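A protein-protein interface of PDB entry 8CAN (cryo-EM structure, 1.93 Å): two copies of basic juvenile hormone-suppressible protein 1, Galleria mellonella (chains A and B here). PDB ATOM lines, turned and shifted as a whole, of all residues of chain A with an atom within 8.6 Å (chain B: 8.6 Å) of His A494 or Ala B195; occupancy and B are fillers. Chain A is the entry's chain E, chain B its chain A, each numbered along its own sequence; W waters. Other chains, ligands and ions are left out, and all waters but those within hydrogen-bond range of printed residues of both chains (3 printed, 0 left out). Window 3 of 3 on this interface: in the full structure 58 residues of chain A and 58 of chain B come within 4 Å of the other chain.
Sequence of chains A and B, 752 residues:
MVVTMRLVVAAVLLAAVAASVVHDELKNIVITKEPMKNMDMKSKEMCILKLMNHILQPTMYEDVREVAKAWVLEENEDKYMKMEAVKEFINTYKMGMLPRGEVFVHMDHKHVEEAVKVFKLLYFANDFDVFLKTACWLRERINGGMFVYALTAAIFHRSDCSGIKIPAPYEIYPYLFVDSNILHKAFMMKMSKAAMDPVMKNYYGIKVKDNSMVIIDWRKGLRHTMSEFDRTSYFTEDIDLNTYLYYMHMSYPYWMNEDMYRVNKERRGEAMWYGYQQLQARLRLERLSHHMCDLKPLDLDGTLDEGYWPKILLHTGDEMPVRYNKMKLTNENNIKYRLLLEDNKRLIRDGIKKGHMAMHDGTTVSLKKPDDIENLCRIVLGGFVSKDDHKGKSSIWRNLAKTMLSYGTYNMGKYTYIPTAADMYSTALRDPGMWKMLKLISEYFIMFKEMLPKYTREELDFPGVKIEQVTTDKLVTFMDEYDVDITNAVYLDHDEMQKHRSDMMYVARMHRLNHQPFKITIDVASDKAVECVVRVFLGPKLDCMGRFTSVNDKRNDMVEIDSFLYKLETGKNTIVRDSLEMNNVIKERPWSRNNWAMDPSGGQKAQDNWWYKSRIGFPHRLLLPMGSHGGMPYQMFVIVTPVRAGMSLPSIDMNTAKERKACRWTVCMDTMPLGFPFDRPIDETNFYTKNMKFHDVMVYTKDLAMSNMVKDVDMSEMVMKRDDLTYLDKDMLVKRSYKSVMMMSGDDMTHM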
ATOM      1  N   GLN A  57      22.603 -31.652   8.698  1.00  0.00           N
ATOM      2  CA  GLN A  57      23.630 -32.462   8.047  1.00  0.00           C
ATOM      3  C   GLN A  57      24.273 -33.356   9.103  1.00  0.00           C
ATOM      4  O   GLN A  57      25.392 -33.086   9.565  1.00  0.00           O
ATOM      5  CB  GLN A  57      24.673 -31.582   7.361  1.00  0.00           C
ATOM      6  CG  GLN A  57      24.116 -30.724   6.237  1.00  0.00           C
ATOM      7  CD  GLN A  57      25.125 -29.722   5.711  1.00  0.00           C
ATOM      8  OE1 GLN A  57      25.366 -28.685   6.328  1.00  0.00           O
ATOM      9  NE2 GLN A  57      25.723 -30.029   4.567  1.00  0.00           N
ATOM     10  N   THR A  59      26.449 -36.022  10.443  1.00  0.00           N
ATOM     11  CA  THR A  59      27.564 -36.888  10.073  1.00  0.00           C
ATOM     12  C   THR A  59      28.847 -36.424  10.752  1.00  0.00           C
ATOM     13  O   THR A  59      28.807 -35.652  11.710  1.00  0.00           O
ATOM     14  CB  THR A  59      27.784 -36.924   8.546  1.00  0.00           C
ATOM     15  OG1 THR A  59      28.970 -37.673   8.250  1.00  0.00           O
ATOM     16  CG2 THR A  59      27.921 -35.518   7.983  1.00  0.00           C
ATOM     17  N   LYS A 190      25.108 -16.719   1.952  1.00  0.00           N
ATOM     18  CA  LYS A 190      25.894 -17.949   1.923  1.00  0.00           C
ATOM     19  C   LYS A 190      26.226 -18.354   0.492  1.00  0.00           C
ATOM     20  O   LYS A 190      27.368 -18.724   0.192  1.00  0.00           O
ATOM     21  CB  LYS A 190      25.133 -19.068   2.637  1.00  0.00           C
ATOM     22  CG  LYS A 190      25.924 -20.357   2.834  1.00  0.00           C
ATOM     23  CD  LYS A 190      27.042 -20.187   3.848  1.00  0.00           C
ATOM     24  CE  LYS A 190      27.611 -21.530   4.284  1.00  0.00           C
ATOM     25  NZ  LYS A 190      28.185 -22.304   3.151  1.00  0.00           N
ATOM     26  N   TYR A 491      23.420 -24.505   5.030  1.00  0.00           N
ATOM     27  CA  TYR A 491      24.041 -25.791   4.749  1.00  0.00           C
ATOM     28  C   TYR A 491      25.526 -25.602   4.470  1.00  0.00           C
ATOM     29  O   TYR A 491      25.927 -24.646   3.798  1.00  0.00           O
ATOM     30  CB  TYR A 491      23.359 -26.472   3.561  1.00  0.00           C
ATOM     31  CG  TYR A 491      21.978 -27.000   3.884  1.00  0.00           C
ATOM     32  CD1 TYR A 491      20.922 -26.132   4.130  1.00  0.00           C
ATOM     33  CD2 TYR A 491      21.732 -28.364   3.942  1.00  0.00           C
ATOM     34  CE1 TYR A 491      19.660 -26.610   4.427  1.00  0.00           C
ATOM     35  CE2 TYR A 491      20.473 -28.850   4.238  1.00  0.00           C
ATOM     36  CZ  TYR A 491      19.440 -27.970   4.479  1.00  0.00           C
ATOM     37  OH  TYR A 491      18.185 -28.450   4.773  1.00  0.00           O
ATOM     38  N   LEU A 492      26.337 -26.519   4.988  1.00  0.00           N
ATOM     39  CA  LEU A 492      27.787 -26.410   4.940  1.00  0.00           C
ATOM     40  C   LEU A 492      28.360 -27.237   3.795  1.00  0.00           C
ATOM     41  O   LEU A 492      27.801 -28.264   3.403  1.00  0.00           O
ATOM     42  CB  LEU A 492      28.403 -26.871   6.262  1.00  0.00           C
ATOM     43  CG  LEU A 492      27.838 -26.230   7.532  1.00  0.00           C
ATOM     44  CD1 LEU A 492      28.480 -26.841   8.766  1.00  0.00           C
ATOM     45  CD2 LEU A 492      28.036 -24.724   7.516  1.00  0.00           C
ATOM     46  N   ASP A 493      29.490 -26.774   3.265  1.00  0.00           N
ATOM     47  CA  ASP A 493      30.225 -27.507   2.248  1.00  0.00           C
ATOM     48  C   ASP A 493      31.143 -28.530   2.917  1.00  0.00           C
ATOM     49  O   ASP A 493      31.230 -28.616   4.143  1.00  0.00           O
ATOM     50  CB  ASP A 493      31.018 -26.544   1.363  1.00  0.00           C
ATOM     51  CG  ASP A 493      32.027 -25.725   2.146  1.00  0.00           C
ATOM     52  OD1 ASP A 493      33.014 -26.308   2.641  1.00  0.00           O
ATOM     53  OD2 ASP A 493      31.834 -24.497   2.263  1.00  0.00           O
ATOM     54  N   HIS A 494      31.848 -29.316   2.099  1.00  0.00           N
ATOM     55  CA  HIS A 494      32.696 -30.370   2.648  1.00  0.00           C
ATOM     56  C   HIS A 494      33.774 -29.798   3.561  1.00  0.00           C
ATOM     57  O   HIS A 494      33.997 -30.310   4.665  1.00  0.00           O
ATOM     58  CB  HIS A 494      33.333 -31.177   1.515  1.00  0.00           C
ATOM     59  CG  HIS A 494      32.417 -32.194   0.908  1.00  0.00           C
ATOM     60  ND1 HIS A 494      31.833 -32.027  -0.328  1.00  0.00           N
ATOM     61  CD2 HIS A 494      31.986 -33.392   1.369  1.00  0.00           C
ATOM     62  CE1 HIS A 494      31.081 -33.078  -0.603  1.00  0.00           C
ATOM     63  NE2 HIS A 494      31.157 -33.921   0.411  1.00  0.00           N
ATOM     64  N   ASP A 495      34.446 -28.732   3.124  1.00  0.00           N
ATOM     65  CA  ASP A 495      35.503 -28.141   3.937  1.00  0.00           C
ATOM     66  C   ASP A 495      34.949 -27.630   5.261  1.00  0.00           C
ATOM     67  O   ASP A 495      35.553 -27.828   6.321  1.00  0.00           O
ATOM     68  CB  ASP A 495      36.187 -27.012   3.165  1.00  0.00           C
ATOM     69  CG  ASP A 495      36.880 -27.503   1.910  1.00  0.00           C
ATOM     70  OD1 ASP A 495      37.349 -28.661   1.902  1.00  0.00           O
ATOM     71  OD2 ASP A 495      36.959 -26.731   0.932  1.00  0.00           O
ATOM     72  N   GLU A 496      33.793 -26.965   5.217  1.00  0.00           N
ATOM     73  CA  GLU A 496      33.159 -26.507   6.449  1.00  0.00           C
ATOM     74  C   GLU A 496      32.751 -27.684   7.326  1.00  0.00           C
ATOM     75  O   GLU A 496      32.881 -27.628   8.554  1.00  0.00           O
ATOM     76  CB  GLU A 496      31.948 -25.635   6.119  1.00  0.00           C
ATOM     77  CG  GLU A 496      32.307 -24.292   5.504  1.00  0.00           C
ATOM     78  CD  GLU A 496      31.087 -23.491   5.095  1.00  0.00           C
ATOM     79  OE1 GLU A 496      30.010 -24.096   4.913  1.00  0.00           O
ATOM     80  OE2 GLU A 496      31.202 -22.256   4.957  1.00  0.00           O
ATOM     81  N   MET A 497      32.253 -28.761   6.714  1.00  0.00           N
ATOM     82  CA  MET A 497      31.851 -29.931   7.487  1.00  0.00           C
ATOM     83  C   MET A 497      33.039 -30.540   8.221  1.00  0.00           C
ATOM     84  O   MET A 497      32.915 -30.955   9.379  1.00  0.00           O
ATOM     85  CB  MET A 497      31.200 -30.965   6.569  1.00  0.00           C
ATOM     86  CG  MET A 497      29.814 -30.573   6.078  1.00  0.00           C
ATOM     87  SD  MET A 497      28.562 -30.618   7.376  1.00  0.00           S
ATOM     88  CE  MET A 497      28.385 -32.383   7.619  1.00  0.00           C
ATOM     89  N   GLN A 498      34.201 -30.604   7.565  1.00  0.00           N
ATOM     90  CA  GLN A 498      35.376 -31.175   8.218  1.00  0.00           C
ATOM     91  C   GLN A 498      35.755 -30.377   9.460  1.00  0.00           C
ATOM     92  O   GLN A 498      36.150 -30.954  10.480  1.00  0.00           O
ATOM     93  CB  GLN A 498      36.552 -31.236   7.244  1.00  0.00           C
ATOM     94  CG  GLN A 498      36.283 -32.057   5.993  1.00  0.00           C
ATOM     95  CD  GLN A 498      37.550 -32.564   5.334  1.00  0.00           C
ATOM     96  OE1 GLN A 498      38.629 -32.531   5.924  1.00  0.00           O
ATOM     97  NE2 GLN A 498      37.425 -33.037   4.099  1.00  0.00           N
ATOM     98  N   LYS A 499      35.646 -29.051   9.393  1.00  0.00           N
ATOM     99  CA  LYS A 499      35.971 -28.193  10.525  1.00  0.00           C
ATOM    100  C   LYS A 499      34.823 -28.059  11.517  1.00  0.00           C
ATOM    101  O   LYS A 499      35.000 -27.418  12.559  1.00  0.00           O
ATOM    102  CB  LYS A 499      36.379 -26.803  10.029  1.00  0.00           C
ATOM    103  CG  LYS A 499      37.560 -26.805   9.074  1.00  0.00           C
ATOM    104  CD  LYS A 499      37.909 -25.395   8.623  1.00  0.00           C
ATOM    105  CE  LYS A 499      39.056 -25.395   7.625  1.00  0.00           C
ATOM    106  NZ  LYS A 499      40.301 -25.981   8.194  1.00  0.00           N
ATOM    107  N   HIS A 500      33.662 -28.641  11.224  1.00  0.00           N
ATOM    108  CA  HIS A 500      32.508 -28.583  12.120  1.00  0.00           C
ATOM    109  C   HIS A 500      32.142 -27.139  12.449  1.00  0.00           C
ATOM    110  O   HIS A 500      31.786 -26.807  13.582  1.00  0.00           O
ATOM    111  CB  HIS A 500      32.772 -29.378  13.401  1.00  0.00           C
ATOM    112  CG  HIS A 500      33.106 -30.817  13.163  1.00  0.00           C
ATOM    113  ND1 HIS A 500      32.155 -31.757  12.828  1.00  0.00           N
ATOM    114  CD2 HIS A 500      34.286 -31.478  13.218  1.00  0.00           C
ATOM    115  CE1 HIS A 500      32.736 -32.935  12.683  1.00  0.00           C
ATOM    116  NE2 HIS A 500      34.028 -32.794  12.915  1.00  0.00           N
ATOM    117  N   ARG A 501      32.230 -26.267  11.448  1.00  0.00           N
ATOM    118  CA  ARG A 501      31.915 -24.860  11.645  1.00  0.00           C
ATOM    119  C   ARG A 501      31.840 -24.172  10.292  1.00  0.00           C
ATOM    120  O   ARG A 501      32.563 -24.531   9.358  1.00  0.00           O
ATOM    121  CB  ARG A 501      32.962 -24.171  12.530  1.00  0.00           C
ATOM    122  CG  ARG A 501      32.660 -22.710  12.837  1.00  0.00           C
ATOM    123  CD  ARG A 501      33.804 -22.046  13.585  1.00  0.00           C
ATOM    124  NE  ARG A 501      35.046 -22.078  12.819  1.00  0.00           N
ATOM    125  CZ  ARG A 501      35.353 -21.227  11.849  1.00  0.00           C
ATOM    126  NH1 ARG A 501      34.525 -20.260  11.487  1.00  0.00           N
ATOM    127  NH2 ARG A 501      36.518 -21.354  11.221  1.00  0.00           N
ATOM    128  N   MET B 188      20.037 -25.088  -1.510  1.00  0.00           N
ATOM    129  CA  MET B 188      20.815 -25.961  -0.637  1.00  0.00           C
ATOM    130  C   MET B 188      22.028 -26.519  -1.369  1.00  0.00           C
ATOM    131  O   MET B 188      23.142 -26.525  -0.831  1.00  0.00           O
ATOM    132  CB  MET B 188      19.933 -27.097  -0.120  1.00  0.00           C
ATOM    133  CG  MET B 188      18.808 -26.635   0.787  1.00  0.00           C
ATOM    134  SD  MET B 188      17.433 -27.800   0.863  1.00  0.00           S
ATOM    135  CE  MET B 188      18.287 -29.319   1.269  1.00  0.00           C
ATOM    136  N   MET B 189      21.832 -26.983  -2.605  1.00  0.00           N
ATOM    137  CA  MET B 189      22.952 -27.509  -3.380  1.00  0.00           C
ATOM    138  C   MET B 189      23.987 -26.424  -3.656  1.00  0.00           C
ATOM    139  O   MET B 189      25.195 -26.675  -3.582  1.00  0.00           O
ATOM    140  CB  MET B 189      22.448 -28.114  -4.689  1.00  0.00           C
ATOM    141  CG  MET B 189      21.578 -29.351  -4.505  1.00  0.00           C
ATOM    142  SD  MET B 189      22.465 -30.757  -3.802  1.00  0.00           S
ATOM    143  CE  MET B 189      23.510 -31.234  -5.176  1.00  0.00           C
ATOM    144  N   LYS B 190      23.532 -25.212  -3.980  1.00  0.00           N
ATOM    145  CA  LYS B 190      24.465 -24.113  -4.218  1.00  0.00           C
ATOM    146  C   LYS B 190      25.270 -23.795  -2.963  1.00  0.00           C
ATOM    147  O   LYS B 190      26.490 -23.607  -3.029  1.00  0.00           O
ATOM    148  CB  LYS B 190      23.701 -22.877  -4.695  1.00  0.00           C
ATOM    149  CG  LYS B 190      24.578 -21.716  -5.150  1.00  0.00           C
ATOM    150  CD  LYS B 190      25.301 -22.028  -6.450  1.00  0.00           C
ATOM    151  CE  LYS B 190      25.905 -20.776  -7.069  1.00  0.00           C
ATOM    152  NZ  LYS B 190      26.903 -20.122  -6.180  1.00  0.00           N
ATOM    153  N   MET B 191      24.602 -23.735  -1.809  1.00  0.00           N
ATOM    154  CA  MET B 191      25.295 -23.422  -0.564  1.00  0.00           C
ATOM    155  C   MET B 191      26.302 -24.507  -0.204  1.00  0.00           C
ATOM    156  O   MET B 191      27.425 -24.206   0.217  1.00  0.00           O
ATOM    157  CB  MET B 191      24.283 -23.237   0.568  1.00  0.00           C
ATOM    158  CG  MET B 191      23.480 -21.947   0.480  1.00  0.00           C
ATOM    159  SD  MET B 191      22.396 -21.697   1.900  1.00  0.00           S
ATOM    160  CE  MET B 191      21.243 -23.051   1.698  1.00  0.00           C
ATOM    161  N   SER B 192      25.922 -25.773  -0.359  1.00  0.00           N
ATOM    162  CA  SER B 192      26.796 -26.885  -0.012  1.00  0.00           C
ATOM    163  C   SER B 192      27.726 -27.284  -1.150  1.00  0.00           C
ATOM    164  O   SER B 192      28.566 -28.170  -0.961  1.00  0.00           O
ATOM    165  CB  SER B 192      25.960 -28.098   0.410  1.00  0.00           C
ATOM    166  OG  SER B 192      25.228 -28.622  -0.684  1.00  0.00           O
ATOM    167  N   LYS B 193      27.603 -26.653  -2.315  1.00  0.00           N
ATOM    168  CA  LYS B 193      28.399 -26.991  -3.491  1.00  0.00           C
ATOM    169  C   LYS B 193      28.327 -28.493  -3.774  1.00  0.00           C
ATOM    170  O   LYS B 193      29.330 -29.163  -4.023  1.00  0.00           O
ATOM    171  CB  LYS B 193      29.848 -26.527  -3.324  1.00  0.00           C
ATOM    172  CG  LYS B 193      29.989 -25.037  -3.063  1.00  0.00           C
ATOM    173  CD  LYS B 193      31.235 -24.461  -3.721  1.00  0.00           C
ATOM    174  CE  LYS B 193      32.504 -25.150  -3.242  1.00  0.00           C
ATOM    175  NZ  LYS B 193      32.678 -25.044  -1.768  1.00  0.00           N
ATOM    176  N   ALA B 194      27.100 -29.011  -3.722  1.00  0.00           N
ATOM    177  CA  ALA B 194      26.815 -30.413  -4.026  1.00  0.00           C
ATOM    178  C   ALA B 194      27.525 -31.347  -3.043  1.00  0.00           C
ATOM    179  O   ALA B 194      28.299 -32.227  -3.425  1.00  0.00           O
ATOM    180  CB  ALA B 194      27.194 -30.741  -5.473  1.00  0.00           C
ATOM    181  N   ALA B 195      27.246 -31.134  -1.758  1.00  0.00           N
ATOM    182  CA  ALA B 195      27.755 -31.986  -0.690  1.00  0.00           C
ATOM    183  C   ALA B 195      26.647 -32.753   0.021  1.00  0.00           C
ATOM    184  O   ALA B 195      26.881 -33.302   1.104  1.00  0.00           O
ATOM    185  CB  ALA B 195      28.545 -31.153   0.320  1.00  0.00           C
ATOM    186  N   MET B 196      25.449 -32.801  -0.556  1.00  0.00           N
ATOM    187  CA  MET B 196      24.333 -33.487   0.079  1.00  0.00           C
ATOM    188  C   MET B 196      24.617 -34.981   0.193  1.00  0.00           C
ATOM    189  O   MET B 196      25.207 -35.590  -0.704  1.00  0.00           O
ATOM    190  CB  MET B 196      23.055 -33.248  -0.725  1.00  0.00           C
ATOM    191  CG  MET B 196      21.780 -33.665  -0.016  1.00  0.00           C
ATOM    192  SD  MET B 196      20.296 -33.101  -0.872  1.00  0.00           S
ATOM    193  CE  MET B 196      20.434 -31.323  -0.686  1.00  0.00           C
ATOM    194  N   ASP B 197      24.192 -35.572   1.309  1.00  0.00           N
ATOM    195  CA  ASP B 197      24.456 -36.977   1.558  1.00  0.00           C
ATOM    196  C   ASP B 197      23.612 -37.857   0.634  1.00  0.00           C
ATOM    197  O   ASP B 197      22.569 -37.429   0.135  1.00  0.00           O
ATOM    198  CB  ASP B 197      24.171 -37.324   3.018  1.00  0.00           C
ATOM    199  CG  ASP B 197      22.718 -37.126   3.394  1.00  0.00           C
ATOM    200  OD1 ASP B 197      21.882 -37.964   2.994  1.00  0.00           O
ATOM    201  OD2 ASP B 197      22.412 -36.134   4.089  1.00  0.00           O
ATOM    202  N   PRO B 198      24.051 -39.096   0.389  1.00  0.00           N
ATOM    203  CA  PRO B 198      23.314 -39.953  -0.558  1.00  0.00           C
ATOM    204  C   PRO B 198      21.857 -40.173  -0.189  1.00  0.00           C
ATOM    205  O   PRO B 198      21.002 -40.218  -1.082  1.00  0.00           O
ATOM    206  CB  PRO B 198      24.108 -41.267  -0.527  1.00  0.00           C
ATOM    207  CG  PRO B 198      25.467 -40.886  -0.064  1.00  0.00           C
ATOM    208  CD  PRO B 198      25.271 -39.752   0.892  1.00  0.00           C
ATOM    209  N   MET B 200      19.658 -38.233   1.404  1.00  0.00           N
ATOM    210  CA  MET B 200      18.824 -37.080   1.084  1.00  0.00           C
ATOM    211  C   MET B 200      18.643 -36.933  -0.422  1.00  0.00           C
ATOM    212  O   MET B 200      17.534 -36.657  -0.897  1.00  0.00           O
ATOM    213  CB  MET B 200      19.439 -35.812   1.673  1.00  0.00           C
ATOM    214  CG  MET B 200      19.470 -35.776   3.196  1.00  0.00           C
ATOM    215  SD  MET B 200      17.847 -35.967   3.955  1.00  0.00           S
ATOM    216  CE  MET B 200      16.929 -34.692   3.101  1.00  0.00           C
ATOM    217  N   LYS B 201      19.720 -37.108  -1.190  1.00  0.00           N
ATOM    218  CA  LYS B 201      19.613 -36.993  -2.641  1.00  0.00           C
ATOM    219  C   LYS B 201      18.685 -38.057  -3.209  1.00  0.00           C
ATOM    220  O   LYS B 201      17.865 -37.772  -4.090  1.00  0.00           O
ATOM    221  CB  LYS B 201      20.999 -37.092  -3.280  1.00  0.00           C
ATOM    222  CG  LYS B 201      21.926 -35.941  -2.927  1.00  0.00           C
ATOM    223  CD  LYS B 201      23.145 -35.898  -3.838  1.00  0.00           C
ATOM    224  CE  LYS B 201      24.007 -37.140  -3.691  1.00  0.00           C
ATOM    225  NZ  LYS B 201      25.215 -37.081  -4.558  1.00  0.00           N
ATOM    226  N   VAL B 208      23.884 -35.326  -9.591  1.00  0.00           N
ATOM    227  CA  VAL B 208      24.902 -34.479 -10.204  1.00  0.00           C
ATOM    228  C   VAL B 208      25.440 -35.219 -11.421  1.00  0.00           C
ATOM    229  O   VAL B 208      25.974 -36.328 -11.293  1.00  0.00           O
ATOM    230  CB  VAL B 208      26.034 -34.138  -9.222  1.00  0.00           C
ATOM    231  CG1 VAL B 208      27.003 -33.150  -9.852  1.00  0.00           C
ATOM    232  CG2 VAL B 208      25.466 -33.583  -7.924  1.00  0.00           C
ATOM    233  N   VAL B 214      23.398 -30.018 -12.017  1.00  0.00           N
ATOM    234  CA  VAL B 214      22.622 -30.500 -10.880  1.00  0.00           C
ATOM    235  C   VAL B 214      21.181 -30.648 -11.342  1.00  0.00           C
ATOM    236  O   VAL B 214      20.563 -29.672 -11.787  1.00  0.00           O
ATOM    237  CB  VAL B 214      22.718 -29.550  -9.674  1.00  0.00           C
ATOM    238  CG1 VAL B 214      21.851 -30.051  -8.526  1.00  0.00           C
ATOM    239  CG2 VAL B 214      24.164 -29.403  -9.227  1.00  0.00           C
ATOM    240  N   MET B 504      28.274 -24.432 -11.914  1.00  0.00           N
ATOM    241  CA  MET B 504      27.399 -25.592 -12.014  1.00  0.00           C
ATOM    242  C   MET B 504      26.029 -25.157 -12.511  1.00  0.00           C
ATOM    243  O   MET B 504      25.495 -24.134 -12.073  1.00  0.00           O
ATOM    244  CB  MET B 504      27.267 -26.295 -10.658  1.00  0.00           C
ATOM    245  CG  MET B 504      28.572 -26.873 -10.133  1.00  0.00           C
ATOM    246  SD  MET B 504      28.877 -28.559 -10.690  1.00  0.00           S
ATOM    247  CE  MET B 504      27.787 -29.470  -9.603  1.00  0.00           C
HETATM  248  O   HOH W   1      31.464 -29.490  -1.152  1.00  0.00           O
HETATM  249  O   HOH W   2      28.324 -21.370  -1.775  1.00  0.00           O
HETATM  250  O   HOH W   3      26.191 -32.898   4.362  1.00  0.00           O
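The backbone carbonyl oxygen (O) of Met B188 sits at hydrogen-bond distance from the side-chain hydroxyl (OG) of Ser B192 (3.0 Å).
The backbone carbonyl oxygen (O) of Met B189 is in hydrogen-bond range of the side-chain hydroxyl (OG) of Ser B192, 3.5 Å away.
The side-chain hydroxyl (OG) of Ser B192 lies within hydrogen-bond range of the backbone NH (N) of Ala B195.
OE1 of Gln A57 lies within hydrogen-bond range of N of Leu A492.
The side-chain carboxylate (OE1) of Glu A496 is in salt-bridge range of the side-chain amino group (NZ) of Lys A190, 3.1 Å away.
The backbone NH of Asp A495 lies within hydrogen-bond range of the side-chain carboxylate of Asp A493.
Lys A190 touches Met B191 (NZ to O, 3.6 Å).
Tyr A491 touches Met B188 (OH to CE, 3.6 Å).
Met B191 touches Tyr A491.
Ser B192 touches Leu A492 (CB to O, 3.5 Å).
O of Ser B192 touches CA of Asp A493, 3.7 Å away.
CB of Asp A493 touches NZ of Lys B193, 3.8 Å away.
Ala B195 touches His A494 (CB to CE1, 3.3 Å).
Of chain B, only Ala B195 (3.3 Å) comes within 4 Å of His A494.
Printed residues of chain A within 4 Å of Ala B195: His A494 (3.3 Å).
Ala B194 touches none of the printed residues of chain A.
Printed residues of chain B within 4 Å of Lys A190: Met B191.
Printed residues of chain A within 4 Å of Ser B192: Leu A492 (3.5 Å) and Asp A493 (3.7 Å).
Glu A496 touches none of the printed residues of chain B.
The nearest residue of chain A that does not touch Ala B195 is Leu A492 (4.3 Å).
Hydrophobic or aromatic side chains of chain B that line the printed part of chain A: Met B188, Met B191 and Ala B195.
Hydrophobic or aromatic side chains of chain A within 4 Å of the printed part of chain B: Tyr A491 and His A494.
Along chain A the printed residues that touch a printed residue of chain B span positions 190 to 494.
Among the printed residues, 7 pairs touch across the chains.
Position printed for both chains: 190.
Of the 7 pairs that touch across the chains among the printed residues, none has its exchanged pair printed and touching as well.
Water W1 lies within hydrogen-bond range of a ring nitrogen (ND1) of His A494 (2.7 Å) and the backbone carbonyl oxygen (O) of Ser B192 (3.2 Å).
Water W3 bridges NE2 of Gln A57 (2.9 Å) and O of Ala B195 (3.4 Å).
Water W2 lies within hydrogen-bond range of the backbone carbonyl oxygen of Lys B190 (3.2 Å) and the backbone carbonyl oxygen of Lys A190 (3.4 Å).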
